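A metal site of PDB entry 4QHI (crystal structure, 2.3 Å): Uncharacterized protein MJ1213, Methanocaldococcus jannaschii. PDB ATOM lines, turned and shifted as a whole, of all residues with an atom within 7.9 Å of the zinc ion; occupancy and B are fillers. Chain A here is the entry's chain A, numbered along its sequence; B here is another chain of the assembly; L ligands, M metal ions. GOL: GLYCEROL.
O of Lys 78 lies close to ND1 of His 73.
ND1 of His 73 lies within hydrogen-bond range of O of Gly 77, at 2.8 Å.
ND1 of His 80 sits close to O of Pro 56 of chain B, at 3.3 Å.
A ring nitrogen (NE2) of His 73 is bound to the zinc ion (1.9 Å).
O2 of the ligand binds the zinc ion (2.0 Å).
NE2 of His 69 is bound to the zinc ion, at 2.0 Å.
NE2 of His 80 is bound to the zinc ion.
The zinc ion has four donor atoms within binding distance.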
ATOM      1  N   ALA A  39       0.154  -0.285  32.532  1.00  0.00           N
ATOM      2  CA  ALA A  39      -1.210   0.192  32.608  1.00  0.00           C
ATOM      3  C   ALA A  39      -2.200  -0.913  32.293  1.00  0.00           C
ATOM      4  O   ALA A  39      -1.821  -1.951  31.750  1.00  0.00           O
ATOM      5  CB  ALA A  39      -1.423   1.345  31.633  1.00  0.00           C
ATOM      6  N   SER A  40      -3.484  -0.645  32.608  1.00  0.00           N
ATOM      7  CA  SER A  40      -4.630  -1.522  32.361  1.00  0.00           C
ATOM      8  C   SER A  40      -5.882  -0.656  32.251  1.00  0.00           C
ATOM      9  O   SER A  40      -5.840   0.508  32.626  1.00  0.00           O
ATOM     10  CB  SER A  40      -4.776  -2.560  33.466  1.00  0.00           C
ATOM     11  OG  SER A  40      -5.191  -1.972  34.689  1.00  0.00           O
ATOM     12  N   ILE A  41      -6.969  -1.203  31.721  1.00  0.00           N
ATOM     13  CA  ILE A  41      -8.228  -0.476  31.608  1.00  0.00           C
ATOM     14  C   ILE A  41      -9.359  -1.395  32.019  1.00  0.00           C
ATOM     15  O   ILE A  41      -9.364  -2.579  31.660  1.00  0.00           O
ATOM     16  CB  ILE A  41      -8.453   0.147  30.173  1.00  0.00           C
ATOM     17  CG1 ILE A  41      -9.672   1.127  30.169  1.00  0.00           C
ATOM     18  CG2 ILE A  41      -8.557  -0.897  29.060  1.00  0.00           C
ATOM     19  CD1 ILE A  41      -9.751   2.073  29.016  1.00  0.00           C
ATOM     20  N   HIS A  69      -3.171   3.797  23.843  1.00  0.00           N
ATOM     21  CA  HIS A  69      -3.365   2.342  23.776  1.00  0.00           C
ATOM     22  C   HIS A  69      -4.626   1.939  24.547  1.00  0.00           C
ATOM     23  O   HIS A  69      -5.472   1.234  24.003  1.00  0.00           O
ATOM     24  CB  HIS A  69      -2.116   1.581  24.307  1.00  0.00           C
ATOM     25  CG  HIS A  69      -2.317   0.079  24.292  1.00  0.00           C
ATOM     26  ND1 HIS A  69      -1.802  -0.711  23.286  1.00  0.00           N
ATOM     27  CD2 HIS A  69      -3.031  -0.707  25.129  1.00  0.00           C
ATOM     28  CE1 HIS A  69      -2.218  -1.936  23.534  1.00  0.00           C
ATOM     29  NE2 HIS A  69      -2.959  -1.990  24.638  1.00  0.00           N
ATOM     30  N   GLU A  70      -4.766   2.429  25.783  1.00  0.00           N
ATOM     31  CA  GLU A  70      -5.914   2.126  26.638  1.00  0.00           C
ATOM     32  C   GLU A  70      -7.228   2.690  26.079  1.00  0.00           C
ATOM     33  O   GLU A  70      -8.252   1.990  26.047  1.00  0.00           O
ATOM     34  CB  GLU A  70      -5.649   2.604  28.061  1.00  0.00           C
ATOM     35  CG  GLU A  70      -4.540   1.853  28.802  1.00  0.00           C
ATOM     36  CD  GLU A  70      -4.333   0.367  28.520  1.00  0.00           C
ATOM     37  OE1 GLU A  70      -5.341  -0.314  28.232  1.00  0.00           O
ATOM     38  OE2 GLU A  70      -3.212  -0.144  28.741  1.00  0.00           O
ATOM     39  N   LEU A  72      -7.901   3.321  22.967  1.00  0.00           N
ATOM     40  CA  LEU A  72      -8.248   2.591  21.731  1.00  0.00           C
ATOM     41  C   LEU A  72      -9.087   1.324  22.043  1.00  0.00           C
ATOM     42  O   LEU A  72      -9.840   0.873  21.190  1.00  0.00           O
ATOM     43  CB  LEU A  72      -7.004   2.234  20.892  1.00  0.00           C
ATOM     44  CG  LEU A  72      -6.465   3.318  19.983  1.00  0.00           C
ATOM     45  CD1 LEU A  72      -5.155   2.906  19.369  1.00  0.00           C
ATOM     46  CD2 LEU A  72      -7.396   3.573  18.838  1.00  0.00           C
ATOM     47  N   HIS A  73      -9.002   0.797  23.284  1.00  0.00           N
ATOM     48  CA  HIS A  73      -9.802  -0.346  23.709  1.00  0.00           C
ATOM     49  C   HIS A  73     -11.263   0.075  23.906  1.00  0.00           C
ATOM     50  O   HIS A  73     -12.147  -0.751  23.734  1.00  0.00           O
ATOM     51  CB  HIS A  73      -9.227  -1.013  24.966  1.00  0.00           C
ATOM     52  CG  HIS A  73      -8.083  -1.922  24.670  1.00  0.00           C
ATOM     53  ND1 HIS A  73      -8.276  -3.119  24.029  1.00  0.00           N
ATOM     54  CD2 HIS A  73      -6.755  -1.767  24.921  1.00  0.00           C
ATOM     55  CE1 HIS A  73      -7.085  -3.676  23.933  1.00  0.00           C
ATOM     56  NE2 HIS A  73      -6.138  -2.886  24.453  1.00  0.00           N
ATOM     57  N   GLY A  77     -12.830  -2.380  21.411  1.00  0.00           N
ATOM     58  CA  GLY A  77     -13.077  -3.534  22.272  1.00  0.00           C
ATOM     59  C   GLY A  77     -11.786  -4.026  22.913  1.00  0.00           C
ATOM     60  O   GLY A  77     -10.744  -3.404  22.727  1.00  0.00           O
ATOM     61  N   LYS A  78     -11.826  -5.147  23.651  1.00  0.00           N
ATOM     62  CA  LYS A  78     -10.643  -5.621  24.386  1.00  0.00           C
ATOM     63  C   LYS A  78      -9.561  -6.302  23.509  1.00  0.00           C
ATOM     64  O   LYS A  78      -8.466  -6.555  24.008  1.00  0.00           O
ATOM     65  CB  LYS A  78     -11.020  -6.557  25.569  1.00  0.00           C
ATOM     66  CG  LYS A  78     -11.884  -7.748  25.235  1.00  0.00           C
ATOM     67  CD  LYS A  78     -12.359  -8.456  26.510  1.00  0.00           C
ATOM     68  CE  LYS A  78     -11.543  -9.687  26.844  1.00  0.00           C
ATOM     69  NZ  LYS A  78     -12.285 -10.618  27.735  1.00  0.00           N
ATOM     70  N   TYR A  79      -9.813  -6.523  22.218  1.00  0.00           N
ATOM     71  CA  TYR A  79      -8.835  -7.190  21.364  1.00  0.00           C
ATOM     72  C   TYR A  79      -8.107  -6.255  20.402  1.00  0.00           C
ATOM     73  O   TYR A  79      -8.685  -5.320  19.852  1.00  0.00           O
ATOM     74  CB  TYR A  79      -9.498  -8.351  20.607  1.00  0.00           C
ATOM     75  CG  TYR A  79     -10.127  -9.349  21.562  1.00  0.00           C
ATOM     76  CD1 TYR A  79      -9.336 -10.124  22.413  1.00  0.00           C
ATOM     77  CD2 TYR A  79     -11.505  -9.454  21.685  1.00  0.00           C
ATOM     78  CE1 TYR A  79      -9.907 -11.026  23.319  1.00  0.00           C
ATOM     79  CE2 TYR A  79     -12.091 -10.332  22.595  1.00  0.00           C
ATOM     80  CZ  TYR A  79     -11.287 -11.126  23.400  1.00  0.00           C
ATOM     81  OH  TYR A  79     -11.855 -12.013  24.287  1.00  0.00           O
ATOM     82  N   HIS A  80      -6.814  -6.539  20.213  1.00  0.00           N
ATOM     83  CA  HIS A  80      -5.932  -5.776  19.348  1.00  0.00           C
ATOM     84  C   HIS A  80      -6.130  -6.191  17.900  1.00  0.00           C
ATOM     85  O   HIS A  80      -5.239  -6.765  17.277  1.00  0.00           O
ATOM     86  CB  HIS A  80      -4.460  -5.949  19.776  1.00  0.00           C
ATOM     87  CG  HIS A  80      -4.210  -5.635  21.207  1.00  0.00           C
ATOM     88  ND1 HIS A  80      -3.741  -6.593  22.091  1.00  0.00           N
ATOM     89  CD2 HIS A  80      -4.407  -4.477  21.875  1.00  0.00           C
ATOM     90  CE1 HIS A  80      -3.671  -5.986  23.264  1.00  0.00           C
ATOM     91  NE2 HIS A  80      -4.029  -4.701  23.173  1.00  0.00           N
ATOM     92  N   PHE A  84      -7.060  -1.504  15.324  1.00  0.00           N
ATOM     93  CA  PHE A  84      -6.430  -1.019  16.568  1.00  0.00           C
ATOM     94  C   PHE A  84      -4.951  -0.732  16.297  1.00  0.00           C
ATOM     95  O   PHE A  84      -4.469   0.391  16.553  1.00  0.00           O
ATOM     96  CB  PHE A  84      -6.616  -2.069  17.688  1.00  0.00           C
ATOM     97  CG  PHE A  84      -6.184  -1.649  19.078  1.00  0.00           C
ATOM     98  CD1 PHE A  84      -4.837  -1.395  19.362  1.00  0.00           C
ATOM     99  CD2 PHE A  84      -7.096  -1.599  20.121  1.00  0.00           C
ATOM    100  CE1 PHE A  84      -4.442  -1.006  20.644  1.00  0.00           C
ATOM    101  CE2 PHE A  84      -6.691  -1.246  21.405  1.00  0.00           C
ATOM    102  CZ  PHE A  84      -5.368  -0.933  21.654  1.00  0.00           C
ATOM    103  N   LEU A  88      -2.981   2.959  16.067  1.00  0.00           N
ATOM    104  CA  LEU A  88      -1.884   3.201  16.993  1.00  0.00           C
ATOM    105  C   LEU A  88      -0.582   3.462  16.216  1.00  0.00           C
ATOM    106  O   LEU A  88       0.180   4.343  16.602  1.00  0.00           O
ATOM    107  CB  LEU A  88      -1.736   2.017  17.960  1.00  0.00           C
ATOM    108  CG  LEU A  88      -0.998   2.310  19.294  1.00  0.00           C
ATOM    109  CD1 LEU A  88      -1.578   3.531  20.052  1.00  0.00           C
ATOM    110  CD2 LEU A  88      -1.024   1.106  20.177  1.00  0.00           C
ATOM    111  N   MET B   1      -4.772 -13.011  25.383  1.00  0.00           N
ATOM    112  CA  MET B   1      -5.328 -12.579  24.095  1.00  0.00           C
ATOM    113  C   MET B   1      -4.436 -13.064  22.941  1.00  0.00           C
ATOM    114  O   MET B   1      -4.941 -13.718  22.018  1.00  0.00           O
ATOM    115  CB  MET B   1      -5.483 -11.054  24.036  1.00  0.00           C
ATOM    116  CG  MET B   1      -6.458 -10.490  25.056  1.00  0.00           C
ATOM    117  SD  MET B   1      -6.336  -8.695  25.142  1.00  0.00           S
ATOM    118  CE  MET B   1      -4.787  -8.497  26.070  1.00  0.00           C
ATOM    119  N   LEU B  55       3.406  -8.020  26.185  1.00  0.00           N
ATOM    120  CA  LEU B  55       2.899  -8.760  25.015  1.00  0.00           C
ATOM    121  C   LEU B  55       1.645  -8.083  24.410  1.00  0.00           C
ATOM    122  O   LEU B  55       1.620  -8.009  23.178  1.00  0.00           O
ATOM    123  CB  LEU B  55       2.633 -10.243  25.349  1.00  0.00           C
ATOM    124  CG  LEU B  55       2.157 -11.165  24.218  1.00  0.00           C
ATOM    125  CD1 LEU B  55       3.201 -11.271  23.089  1.00  0.00           C
ATOM    126  CD2 LEU B  55       1.840 -12.553  24.746  1.00  0.00           C
ATOM    127  N   PRO B  56       0.673  -7.498  25.168  1.00  0.00           N
ATOM    128  CA  PRO B  56      -0.460  -6.805  24.528  1.00  0.00           C
ATOM    129  C   PRO B  56      -0.066  -5.604  23.636  1.00  0.00           C
ATOM    130  O   PRO B  56      -0.816  -5.287  22.702  1.00  0.00           O
ATOM    131  CB  PRO B  56      -1.302  -6.327  25.707  1.00  0.00           C
ATOM    132  CG  PRO B  56      -0.992  -7.301  26.784  1.00  0.00           C
ATOM    133  CD  PRO B  56       0.475  -7.524  26.641  1.00  0.00           C
ATOM    134  N   TYR B  57       1.118  -4.976  23.856  1.00  0.00           N
ATOM    135  CA  TYR B  57       1.586  -3.856  23.020  1.00  0.00           C
ATOM    136  C   TYR B  57       2.220  -4.321  21.734  1.00  0.00           C
ATOM    137  O   TYR B  57       2.468  -3.507  20.837  1.00  0.00           O
ATOM    138  CB  TYR B  57       2.660  -3.029  23.744  1.00  0.00           C
ATOM    139  CG  TYR B  57       2.183  -2.267  24.957  1.00  0.00           C
ATOM    140  CD1 TYR B  57       1.414  -1.116  24.817  1.00  0.00           C
ATOM    141  CD2 TYR B  57       2.552  -2.645  26.235  1.00  0.00           C
ATOM    142  CE1 TYR B  57       0.969  -0.402  25.937  1.00  0.00           C
ATOM    143  CE2 TYR B  57       2.128  -1.945  27.359  1.00  0.00           C
ATOM    144  CZ  TYR B  57       1.327  -0.818  27.197  1.00  0.00           C
ATOM    145  OH  TYR B  57       0.906  -0.123  28.312  1.00  0.00           O
ATOM    146  N   LEU B  58       2.556  -5.622  21.639  1.00  0.00           N
ATOM    147  CA  LEU B  58       3.335  -6.116  20.520  1.00  0.00           C
ATOM    148  C   LEU B  58       2.539  -6.601  19.308  1.00  0.00           C
ATOM    149  O   LEU B  58       1.684  -7.479  19.406  1.00  0.00           O
ATOM    150  CB  LEU B  58       4.264  -7.249  21.002  1.00  0.00           C
ATOM    151  CG  LEU B  58       5.235  -6.965  22.162  1.00  0.00           C
ATOM    152  CD1 LEU B  58       6.021  -8.226  22.515  1.00  0.00           C
ATOM    153  CD2 LEU B  58       6.172  -5.816  21.815  1.00  0.00           C
HETATM  154  C1  GOL L   1      -2.512  -3.806  27.877  1.00  0.00           C
HETATM  155  O1  GOL L   1      -2.118  -2.669  28.627  1.00  0.00           O
HETATM  156  C2  GOL L   1      -3.907  -3.638  27.308  1.00  0.00           C
HETATM  157  O2  GOL L   1      -4.175  -4.670  26.357  1.00  0.00           O
HETATM  158  C3  GOL L   1      -4.934  -3.671  28.419  1.00  0.00           C
HETATM  159  O3  GOL L   1      -6.036  -2.831  28.125  1.00  0.00           O
HETATM  160 ZN    ZN M   1      -4.338  -3.465  24.758  1.00  0.00          ZN
